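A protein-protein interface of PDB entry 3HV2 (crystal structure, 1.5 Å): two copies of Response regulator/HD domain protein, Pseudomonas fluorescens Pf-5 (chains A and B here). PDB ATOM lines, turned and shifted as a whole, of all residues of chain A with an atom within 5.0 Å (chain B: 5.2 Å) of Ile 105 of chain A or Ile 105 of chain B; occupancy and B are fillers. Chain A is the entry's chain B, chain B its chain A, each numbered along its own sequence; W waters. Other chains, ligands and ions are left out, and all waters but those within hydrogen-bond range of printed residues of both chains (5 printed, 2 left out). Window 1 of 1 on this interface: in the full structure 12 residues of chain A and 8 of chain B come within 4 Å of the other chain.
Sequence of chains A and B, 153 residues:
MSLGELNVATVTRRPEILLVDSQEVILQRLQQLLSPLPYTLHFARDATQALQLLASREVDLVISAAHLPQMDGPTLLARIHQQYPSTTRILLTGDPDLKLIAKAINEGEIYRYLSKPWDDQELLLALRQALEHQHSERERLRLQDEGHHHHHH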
ATOM      1  N   ILE A 101     -28.156  22.043   9.686  1.00  0.00           N
ATOM      2  CA  ILE A 101     -26.858  21.470  10.038  1.00  0.00           C
ATOM      3  C   ILE A 101     -26.753  20.050   9.489  1.00  0.00           C
ATOM      4  O   ILE A 101     -25.713  19.667   8.912  1.00  0.00           O
ATOM      5  CB  ILE A 101     -26.576  21.441  11.569  1.00  0.00           C
ATOM      6  CG1 ILE A 101     -26.978  22.745  12.274  1.00  0.00           C
ATOM      7  CG2 ILE A 101     -25.106  21.082  11.846  1.00  0.00           C
ATOM      8  CD1 ILE A 101     -26.603  24.042  11.609  1.00  0.00           C
ATOM      9  N   ALA A 102     -27.822  19.266   9.612  1.00  0.00           N
ATOM     10  CA  ALA A 102     -27.790  17.885   9.154  1.00  0.00           C
ATOM     11  C   ALA A 102     -27.560  17.814   7.653  1.00  0.00           C
ATOM     12  O   ALA A 102     -26.799  16.975   7.166  1.00  0.00           O
ATOM     13  CB  ALA A 102     -29.101  17.158   9.520  1.00  0.00           C
ATOM     14  N   LYS A 103     -28.200  18.705   6.888  1.00  0.00           N
ATOM     15  CA  LYS A 103     -27.986  18.711   5.463  1.00  0.00           C
ATOM     16  C   LYS A 103     -26.557  19.163   5.132  1.00  0.00           C
ATOM     17  O   LYS A 103     -25.894  18.653   4.206  1.00  0.00           O
ATOM     18  CB  LYS A 103     -28.991  19.650   4.786  1.00  0.00           C
ATOM     19  CG  LYS A 103     -28.849  19.704   3.302  1.00  0.00           C
ATOM     20  CD  LYS A 103     -30.066  20.396   2.696  1.00  0.00           C
ATOM     21  CE  LYS A 103     -29.928  20.515   1.210  1.00  0.00           C
ATOM     22  NZ  LYS A 103     -31.219  21.131   0.705  1.00  0.00           N
ATOM     23  N   ALA A 104     -26.079  20.136   5.909  1.00  0.00           N
ATOM     24  CA  ALA A 104     -24.715  20.609   5.677  1.00  0.00           C
ATOM     25  C   ALA A 104     -23.696  19.474   5.913  1.00  0.00           C
ATOM     26  O   ALA A 104     -22.671  19.427   5.205  1.00  0.00           O
ATOM     27  CB  ALA A 104     -24.416  21.858   6.539  1.00  0.00           C
ATOM     28  N   ILE A 105     -23.960  18.571   6.863  1.00  0.00           N
ATOM     29  CA  ILE A 105     -23.087  17.408   7.071  1.00  0.00           C
ATOM     30  C   ILE A 105     -23.292  16.396   5.930  1.00  0.00           C
ATOM     31  O   ILE A 105     -22.359  16.072   5.176  1.00  0.00           O
ATOM     32  CB  ILE A 105     -23.416  16.724   8.397  1.00  0.00           C
ATOM     33  CG1 ILE A 105     -23.090  17.647   9.563  1.00  0.00           C
ATOM     34  CG2 ILE A 105     -22.653  15.386   8.508  1.00  0.00           C
ATOM     35  CD1 ILE A 105     -23.696  17.132  10.898  1.00  0.00           C
ATOM     36  N   ASN A 106     -24.537  15.949   5.752  1.00  0.00           N
ATOM     37  CA  ASN A 106     -24.757  14.750   4.946  1.00  0.00           C
ATOM     38  C   ASN A 106     -24.685  14.987   3.463  1.00  0.00           C
ATOM     39  O   ASN A 106     -24.432  14.060   2.691  1.00  0.00           O
ATOM     40  CB  ASN A 106     -26.092  14.106   5.326  1.00  0.00           C
ATOM     41  CG  ASN A 106     -26.084  13.569   6.742  1.00  0.00           C
ATOM     42  OD1 ASN A 106     -25.045  13.189   7.250  1.00  0.00           O
ATOM     43  ND2 ASN A 106     -27.243  13.561   7.395  1.00  0.00           N
ATOM     44  N   GLU A 107     -24.972  16.223   3.047  1.00  0.00           N
ATOM     45  CA  GLU A 107     -24.908  16.595   1.626  1.00  0.00           C
ATOM     46  C   GLU A 107     -23.789  17.612   1.362  1.00  0.00           C
ATOM     47  O   GLU A 107     -23.185  17.595   0.307  1.00  0.00           O
ATOM     48  CB  GLU A 107     -26.262  17.164   1.163  1.00  0.00           C
ATOM     49  CG  GLU A 107     -27.369  16.120   1.254  1.00  0.00           C
ATOM     50  CD  GLU A 107     -28.665  16.662   0.712  1.00  0.00           C
ATOM     51  OE1 GLU A 107     -28.642  17.278  -0.373  1.00  0.00           O
ATOM     52  OE2 GLU A 107     -29.690  16.495   1.391  1.00  0.00           O
ATOM     53  N   GLY A 108     -23.527  18.504   2.309  1.00  0.00           N
ATOM     54  CA  GLY A 108     -22.464  19.487   2.127  1.00  0.00           C
ATOM     55  C   GLY A 108     -21.092  18.994   2.549  1.00  0.00           C
ATOM     56  O   GLY A 108     -20.082  19.606   2.195  1.00  0.00           O
ATOM     57  N   GLU A 109     -21.054  17.931   3.350  1.00  0.00           N
ATOM     58  CA  GLU A 109     -19.779  17.418   3.926  1.00  0.00           C
ATOM     59  C   GLU A 109     -18.904  18.553   4.466  1.00  0.00           C
ATOM     60  O   GLU A 109     -17.705  18.652   4.151  1.00  0.00           O
ATOM     61  CB  GLU A 109     -19.035  16.505   2.939  1.00  0.00           C
ATOM     62  CG  GLU A 109     -19.927  15.292   2.634  1.00  0.00           C
ATOM     63  CD  GLU A 109     -19.243  14.192   1.856  1.00  0.00           C
ATOM     64  OE1 GLU A 109     -18.041  14.288   1.558  1.00  0.00           O
ATOM     65  OE2 GLU A 109     -19.971  13.223   1.556  1.00  0.00           O
ATOM     66  N   ILE A 110     -19.534  19.421   5.253  1.00  0.00           N
ATOM     67  CA  ILE A 110     -18.794  20.539   5.844  1.00  0.00           C
ATOM     68  C   ILE A 110     -17.670  20.057   6.754  1.00  0.00           C
ATOM     69  O   ILE A 110     -17.793  19.022   7.445  1.00  0.00           O
ATOM     70  CB  ILE A 110     -19.700  21.573   6.595  1.00  0.00           C
ATOM     71  CG1 ILE A 110     -20.560  20.858   7.653  1.00  0.00           C
ATOM     72  CG2 ILE A 110     -20.558  22.378   5.585  1.00  0.00           C
ATOM     73  CD1 ILE A 110     -21.204  21.815   8.657  1.00  0.00           C
ATOM     74  N   TYR A 111     -16.605  20.856   6.771  1.00  0.00           N
ATOM     75  CA  TYR A 111     -15.459  20.584   7.615  1.00  0.00           C
ATOM     76  C   TYR A 111     -15.671  21.129   9.010  1.00  0.00           C
ATOM     77  O   TYR A 111     -15.251  20.511  10.013  1.00  0.00           O
ATOM     78  CB  TYR A 111     -14.201  21.191   6.963  1.00  0.00           C
ATOM     79  CG  TYR A 111     -12.895  20.824   7.639  1.00  0.00           C
ATOM     80  CD1 TYR A 111     -12.463  19.511   7.656  1.00  0.00           C
ATOM     81  CD2 TYR A 111     -12.104  21.803   8.228  1.00  0.00           C
ATOM     82  CE1 TYR A 111     -11.246  19.155   8.295  1.00  0.00           C
ATOM     83  CE2 TYR A 111     -10.884  21.457   8.866  1.00  0.00           C
ATOM     84  CZ  TYR A 111     -10.479  20.148   8.874  1.00  0.00           C
ATOM     85  OH  TYR A 111      -9.287  19.810   9.495  1.00  0.00           O
ATOM     86  N   ARG A 112     -16.288  22.318   9.095  1.00  0.00           N
ATOM     87  CA  ARG A 112     -16.575  22.921  10.392  1.00  0.00           C
ATOM     88  C   ARG A 112     -17.936  23.610  10.372  1.00  0.00           C
ATOM     89  O   ARG A 112     -18.401  24.037   9.296  1.00  0.00           O
ATOM     90  CB  ARG A 112     -15.547  23.992  10.793  1.00  0.00           C
ATOM     91  CG  ARG A 112     -14.096  23.542  10.911  1.00  0.00           C
ATOM     92  CD  ARG A 112     -13.903  22.709  12.195  1.00  0.00           C
ATOM     93  NE  ARG A 112     -12.524  22.287  12.375  1.00  0.00           N
ATOM     94  CZ  ARG A 112     -12.036  21.096  12.028  1.00  0.00           C
ATOM     95  NH1 ARG A 112     -12.776  20.169  11.422  1.00  0.00           N
ATOM     96  NH2 ARG A 112     -10.777  20.793  12.323  1.00  0.00           N
ATOM     97  N   TYR A 113     -18.557  23.684  11.558  1.00  0.00           N
ATOM     98  CA  TYR A 113     -19.801  24.436  11.769  1.00  0.00           C
ATOM     99  C   TYR A 113     -19.524  25.384  12.934  1.00  0.00           C
ATOM    100  O   TYR A 113     -19.139  24.928  14.030  1.00  0.00           O
ATOM    101  CB  TYR A 113     -20.983  23.502  12.138  1.00  0.00           C
ATOM    102  CG  TYR A 113     -22.084  24.162  12.967  1.00  0.00           C
ATOM    103  CD1 TYR A 113     -22.674  25.376  12.593  1.00  0.00           C
ATOM    104  CD2 TYR A 113     -22.546  23.540  14.117  1.00  0.00           C
ATOM    105  CE1 TYR A 113     -23.682  25.960  13.379  1.00  0.00           C
ATOM    106  CE2 TYR A 113     -23.536  24.125  14.910  1.00  0.00           C
ATOM    107  CZ  TYR A 113     -24.071  25.342  14.536  1.00  0.00           C
ATOM    108  OH  TYR A 113     -25.062  25.916  15.316  1.00  0.00           O
ATOM    109  N   ILE B 101     -23.576  18.236  18.518  1.00  0.00           N
ATOM    110  CA  ILE B 101     -23.454  18.044  17.065  1.00  0.00           C
ATOM    111  C   ILE B 101     -22.225  18.793  16.546  1.00  0.00           C
ATOM    112  O   ILE B 101     -21.425  18.280  15.744  1.00  0.00           O
ATOM    113  CB  ILE B 101     -24.728  18.527  16.292  1.00  0.00           C
ATOM    114  CG1 ILE B 101     -25.990  17.807  16.795  1.00  0.00           C
ATOM    115  CG2 ILE B 101     -24.571  18.374  14.769  1.00  0.00           C
ATOM    116  CD1 ILE B 101     -25.919  16.272  16.794  1.00  0.00           C
ATOM    117  N   ALA B 102     -22.042  20.031  17.015  1.00  0.00           N
ATOM    118  CA  ALA B 102     -20.881  20.811  16.602  1.00  0.00           C
ATOM    119  C   ALA B 102     -19.553  20.149  16.960  1.00  0.00           C
ATOM    120  O   ALA B 102     -18.618  20.199  16.164  1.00  0.00           O
ATOM    121  CB  ALA B 102     -20.932  22.246  17.172  1.00  0.00           C
ATOM    122  N   LYS B 103     -19.456  19.536  18.114  1.00  0.00           N
ATOM    123  CA  LYS B 103     -18.295  18.813  18.450  1.00  0.00           C
ATOM    124  C   LYS B 103     -18.042  17.600  17.550  1.00  0.00           C
ATOM    125  O   LYS B 103     -16.943  17.301  17.240  1.00  0.00           O
ATOM    126  CB  LYS B 103     -18.314  18.415  19.941  1.00  0.00           C
ATOM    127  CG  LYS B 103     -17.094  17.721  20.396  1.00  0.00           C
ATOM    128  CD  LYS B 103     -17.219  17.310  21.839  1.00  0.00           C
ATOM    129  CE  LYS B 103     -16.994  18.425  22.713  1.00  0.00           C
ATOM    130  NZ  LYS B 103     -16.709  17.897  24.068  1.00  0.00           N
ATOM    131  N   ALA B 104     -19.146  16.953  17.203  1.00  0.00           N
ATOM    132  CA  ALA B 104     -19.043  15.805  16.291  1.00  0.00           C
ATOM    133  C   ALA B 104     -18.534  16.209  14.915  1.00  0.00           C
ATOM    134  O   ALA B 104     -17.802  15.426  14.271  1.00  0.00           O
ATOM    135  CB  ALA B 104     -20.389  15.088  16.194  1.00  0.00           C
ATOM    136  N   ILE B 105     -18.929  17.408  14.448  1.00  0.00           N
ATOM    137  CA  ILE B 105     -18.409  17.954  13.190  1.00  0.00           C
ATOM    138  C   ILE B 105     -16.963  18.453  13.335  1.00  0.00           C
ATOM    139  O   ILE B 105     -16.085  18.089  12.552  1.00  0.00           O
ATOM    140  CB  ILE B 105     -19.275  19.139  12.714  1.00  0.00           C
ATOM    141  CG1 ILE B 105     -20.717  18.688  12.472  1.00  0.00           C
ATOM    142  CG2 ILE B 105     -18.661  19.819  11.468  1.00  0.00           C
ATOM    143  CD1 ILE B 105     -21.644  19.867  12.355  1.00  0.00           C
ATOM    144  N   ASN B 106     -16.727  19.272  14.355  1.00  0.00           N
ATOM    145  CA  ASN B 106     -15.485  20.024  14.410  1.00  0.00           C
ATOM    146  C   ASN B 106     -14.321  19.273  14.990  1.00  0.00           C
ATOM    147  O   ASN B 106     -13.171  19.587  14.685  1.00  0.00           O
ATOM    148  CB  ASN B 106     -15.673  21.307  15.191  1.00  0.00           C
ATOM    149  CG  ASN B 106     -16.686  22.247  14.554  1.00  0.00           C
ATOM    150  OD1 ASN B 106     -17.013  22.117  13.378  1.00  0.00           O
ATOM    151  ND2 ASN B 106     -17.180  23.205  15.337  1.00  0.00           N
ATOM    152  N   GLU B 107     -14.622  18.296  15.834  1.00  0.00           N
ATOM    153  CA  GLU B 107     -13.587  17.483  16.456  1.00  0.00           C
ATOM    154  C   GLU B 107     -13.738  16.036  15.989  1.00  0.00           C
ATOM    155  O   GLU B 107     -12.754  15.409  15.617  1.00  0.00           O
ATOM    156  CB  GLU B 107     -13.663  17.594  17.979  1.00  0.00           C
ATOM    157  CG  GLU B 107     -13.371  19.040  18.466  1.00  0.00           C
ATOM    158  CD  GLU B 107     -13.773  19.283  19.930  1.00  0.00           C
ATOM    159  OE1 GLU B 107     -13.847  18.322  20.725  1.00  0.00           O
ATOM    160  OE2 GLU B 107     -13.988  20.468  20.273  1.00  0.00           O
ATOM    161  N   GLY B 108     -14.972  15.533  15.936  1.00  0.00           N
ATOM    162  CA  GLY B 108     -15.207  14.161  15.461  1.00  0.00           C
ATOM    163  C   GLY B 108     -15.046  13.998  13.956  1.00  0.00           C
ATOM    164  O   GLY B 108     -14.819  12.879  13.471  1.00  0.00           O
ATOM    165  N   GLU B 109     -15.209  15.093  13.215  1.00  0.00           N
ATOM    166  CA  GLU B 109     -15.182  15.086  11.731  1.00  0.00           C
ATOM    167  C   GLU B 109     -16.013  13.931  11.170  1.00  0.00           C
ATOM    168  O   GLU B 109     -15.570  13.139  10.322  1.00  0.00           O
ATOM    169  CB  GLU B 109     -13.747  15.141  11.158  1.00  0.00           C
ATOM    170  CG  GLU B 109     -13.085  16.463  11.588  1.00  0.00           C
ATOM    171  CD  GLU B 109     -11.754  16.729  10.944  1.00  0.00           C
ATOM    172  OE1 GLU B 109     -11.349  15.954  10.061  1.00  0.00           O
ATOM    173  OE2 GLU B 109     -11.103  17.715  11.370  1.00  0.00           O
ATOM    174  N   ILE B 110     -17.247  13.855  11.646  1.00  0.00           N
ATOM    175  CA  ILE B 110     -18.112  12.765  11.187  1.00  0.00           C
ATOM    176  C   ILE B 110     -18.433  12.843   9.706  1.00  0.00           C
ATOM    177  O   ILE B 110     -18.575  13.945   9.148  1.00  0.00           O
ATOM    178  CB  ILE B 110     -19.409  12.673  12.014  1.00  0.00           C
ATOM    179  CG1 ILE B 110     -20.184  13.993  11.969  1.00  0.00           C
ATOM    180  CG2 ILE B 110     -19.086  12.245  13.467  1.00  0.00           C
ATOM    181  CD1 ILE B 110     -21.551  13.882  12.620  1.00  0.00           C
ATOM    182  N   TYR B 111     -18.589  11.675   9.089  1.00  0.00           N
ATOM    183  CA  TYR B 111     -18.961  11.642   7.691  1.00  0.00           C
ATOM    184  C   TYR B 111     -20.468  11.819   7.486  1.00  0.00           C
ATOM    185  O   TYR B 111     -20.896  12.472   6.504  1.00  0.00           O
ATOM    186  CB  TYR B 111     -18.504  10.324   7.075  1.00  0.00           C
ATOM    187  CG  TYR B 111     -18.628  10.255   5.592  1.00  0.00           C
ATOM    188  CD1 TYR B 111     -17.905  11.113   4.781  1.00  0.00           C
ATOM    189  CD2 TYR B 111     -19.434   9.276   4.984  1.00  0.00           C
ATOM    190  CE1 TYR B 111     -18.036  11.065   3.372  1.00  0.00           C
ATOM    191  CE2 TYR B 111     -19.521   9.211   3.576  1.00  0.00           C
ATOM    192  CZ  TYR B 111     -18.818  10.093   2.813  1.00  0.00           C
ATOM    193  OH  TYR B 111     -18.894  10.015   1.430  1.00  0.00           O
ATOM    194  N   ARG B 112     -21.261  11.188   8.367  1.00  0.00           N
ATOM    195  CA  ARG B 112     -22.704  11.324   8.328  1.00  0.00           C
ATOM    196  C   ARG B 112     -23.261  11.470   9.725  1.00  0.00           C
ATOM    197  O   ARG B 112     -22.651  11.007  10.722  1.00  0.00           O
ATOM    198  CB  ARG B 112     -23.371  10.103   7.688  1.00  0.00           C
ATOM    199  CG  ARG B 112     -22.993   9.860   6.221  1.00  0.00           C
ATOM    200  CD  ARG B 112     -23.710  10.877   5.287  1.00  0.00           C
ATOM    201  NE  ARG B 112     -23.396  10.635   3.875  1.00  0.00           N
ATOM    202  CZ  ARG B 112     -22.408  11.218   3.185  1.00  0.00           C
ATOM    203  NH1 ARG B 112     -21.552  12.062   3.774  1.00  0.00           N
ATOM    204  NH2 ARG B 112     -22.235  10.918   1.888  1.00  0.00           N
ATOM    205  N   TYR B 113     -24.434  12.092   9.781  1.00  0.00           N
ATOM    206  CA  TYR B 113     -25.193  12.235  11.033  1.00  0.00           C
ATOM    207  C   TYR B 113     -26.539  11.566  10.801  1.00  0.00           C
ATOM    208  O   TYR B 113     -27.204  11.831   9.780  1.00  0.00           O
ATOM    209  CB  TYR B 113     -25.387  13.724  11.399  1.00  0.00           C
ATOM    210  CG  TYR B 113     -26.637  13.962  12.193  1.00  0.00           C
ATOM    211  CD1 TYR B 113     -26.692  13.674  13.555  1.00  0.00           C
ATOM    212  CD2 TYR B 113     -27.794  14.421  11.555  1.00  0.00           C
ATOM    213  CE1 TYR B 113     -27.895  13.880  14.276  1.00  0.00           C
ATOM    214  CE2 TYR B 113     -28.975  14.633  12.263  1.00  0.00           C
ATOM    215  CZ  TYR B 113     -29.012  14.358  13.612  1.00  0.00           C
ATOM    216  OH  TYR B 113     -30.211  14.566  14.279  1.00  0.00           O
HETATM  217  O   HOH W   1     -17.447  12.030   0.162  1.00  0.00           O
HETATM  218  O   HOH W   2     -22.542  13.984   0.598  1.00  0.00           O
HETATM  219  O   HOH W   3     -29.793  11.754   8.690  1.00  0.00           O
HETATM  220  O   HOH W   4     -10.843  18.081  14.102  1.00  0.00           O
HETATM  221  O   HOH W   5      -8.802  17.107   9.579  1.00  0.00           O
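Among the printed residues, pairs that only touch across the chains: Asn 106 of chain A with Arg 112 of chain B, Tyr 111 of chain A with Ile 105 of chain B, Ala 102 of chain A with Tyr 113 of chain B, Tyr 113 of chain A with Ala 102 of chain B, Tyr 113 of chain A with Ile 105 of chain B, Ile 101 of chain A with Ile 105 of chain B, Ile 105 of chain A with Ile 105 of chain B, Ile 105 of chain A with Tyr 113 of chain B, Arg 112 of chain A with Ile 105 of chain B and Ile 105 of chain A with Tyr 111 of chain B.
Water W1 bridges the side-chain carboxylate of Glu 109 of chain A (2.7 Å) and the side-chain hydroxyl of Tyr 111 of chain B (2.8 Å).
Water W5 bridges OH of Tyr 111 of chain A (2.7 Å) and OE1 of Glu 109 of chain B (2.8 Å).
Water W4 lies within hydrogen-bond range of the side-chain carboxylate (OE2) of Glu 109 of chain B (2.8 Å), the backbone carbonyl oxygen (O) of Asn 106 of chain B (2.8 Å) and the guanidinium group (NH2) of Arg 112 of chain A (3.2 Å).
Water W3 lies within hydrogen-bond range of the backbone carbonyl oxygen (O) of Tyr 113 of chain B (2.8 Å) and the side-chain amide nitrogen (ND2) of Asn 106 of chain A (3.4 Å).
Water W2 lies within hydrogen-bond range of the backbone carbonyl oxygen of Asn 106 of chain A, the side-chain carboxylate of Glu 109 of chain A and the guanidinium group of Arg 112 of chain B.
Printed residues of chain B that touch a printed residue of chain A: Ala 102, Ile 105, Asn 106, Glu 109, Tyr 111, Arg 112 and Tyr 113.
Hydrophobic or aromatic side chains of chain B within 4 Å of the printed part of chain A: Ala 102, Ile 105, Tyr 111 and Tyr 113.
Of the 13 printed residues of chain A, 8 touch a printed residue of chain B.
Printed residues of chain A that touch a printed residue of chain B: Ile 101, Ala 102, Ile 105, Asn 106, Glu 109, Tyr 111, Arg 112 and Tyr 113.
Hydrophobic or aromatic side chains of chain A that line the printed part of chain B: Ile 101, Ala 102, Ile 105, Tyr 111 and Tyr 113.
Among the printed residues, 17 pairs touch across the chains.
Of the printed residues of chain B, Ala 102 of chain A touches Tyr 113 (3.7 Å).
Ile 105 of chain A touches just these residues of chain B: Ile 105 (3.7 Å), Tyr 111 (3.9 Å) and Tyr 113 (3.8 Å).
Ile 110 of chain A touches none of the printed residues of chain B.
Printed residues of chain B within 4 Å of Arg 112 of chain A: Ile 105, Asn 106 and Glu 109.
Of the printed residues of chain B, Tyr 113 of chain A touches Ala 102 (3.7 Å), Ile 105 (3.7 Å) and Asn 106 (2.9 Å).
Of the printed residues of chain A, Ile 105 of chain B touches Ile 101 (3.7 Å), Ile 105 (3.7 Å), Tyr 111 (3.6 Å), Arg 112 (3.9 Å) and Tyr 113 (3.7 Å).
Of the printed residues of chain A, Glu 109 of chain B touches Tyr 111 (3.3 Å) and Arg 112 (3.0 Å).
Of the printed residues of chain A, Tyr 111 of chain B touches Ile 105 (3.9 Å) and Glu 109 (3.4 Å).
The nearest printed residue of chain B that does not touch Ile 105 of chain A is Arg 112 of chain B (4.1 Å).
The nearest printed residue of chain A that does not touch Ile 105 of chain B is Ile 110 of chain A (4.2 Å).
The nearest printed residue of chain B that does not touch Asn 106 of chain A is Tyr 111 of chain B (4.3 Å).
Ile 105 of chain A touches Tyr 111 of chain B, and with the chains exchanged Tyr 111 of chain A touches Ile 105 of chain B.
Ile 105 of chain A touches Tyr 113 of chain B, and with the chains exchanged Tyr 113 of chain A touches Ile 105 of chain B.
Asn 106 of chain A touches Arg 112 of chain B, and with the chains exchanged Arg 112 of chain A touches Asn 106 of chain B.
Glu 109 of chain A touches Tyr 111 of chain B, and with the chains exchanged Tyr 111 of chain A touches Glu 109 of chain B.
The backbone carbonyl oxygen (O) of Asn 106 of chain B lies close to the guanidinium group (NH1) of Arg 112 of chain A (3.3 Å).
The side-chain amide oxygen of Asn 106 of chain B is in hydrogen-bond range of the backbone NH of Tyr 113 of chain A (2.9 Å).
OE2 of Glu 109 of chain B is in hydrogen-bond range of OH of Tyr 111 of chain A, 3.3 Å away.
OE2 of Glu 109 of chain B is in salt-bridge range of NH1 of Arg 112 of chain A.
OH of Tyr 111 of chain B sits at hydrogen-bond distance from OE2 of Glu 109 of chain A (3.4 Å).
The guanidinium group (NH1) of Arg 112 of chain B lies within salt-bridge range of the side-chain carboxylate (OE2) of Glu 109 of chain A (3.0 Å).
The backbone NH of Tyr 113 of chain B lies within hydrogen-bond range of the side-chain amide oxygen of Asn 106 of chain A, 2.8 Å away.
ND2 of Asn 106 of chain B lies close to O of Ala 102 of chain B (3.4 Å).
O of Ala 104 of chain B sits at hydrogen-bond distance from N of Glu 109 of chain B (2.8 Å).
OH of Tyr 111 of chain B is in hydrogen-bond range of NH2 of Arg 112 of chain B (3.5 Å).
The side-chain amide nitrogen (ND2) of Asn 106 of chain A sits at hydrogen-bond distance from the backbone carbonyl oxygen (O) of Ala 102 of chain A, at 3.5 Å.
The backbone carbonyl oxygen (O) of Ala 104 of chain A lies within hydrogen-bond range of the backbone NH (N) of Glu 109 of chain A.
The guanidinium group (NH2) of Arg 112 of chain A is in hydrogen-bond range of the side-chain hydroxyl (OH) of Tyr 111 of chain A, 3.3 Å away.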
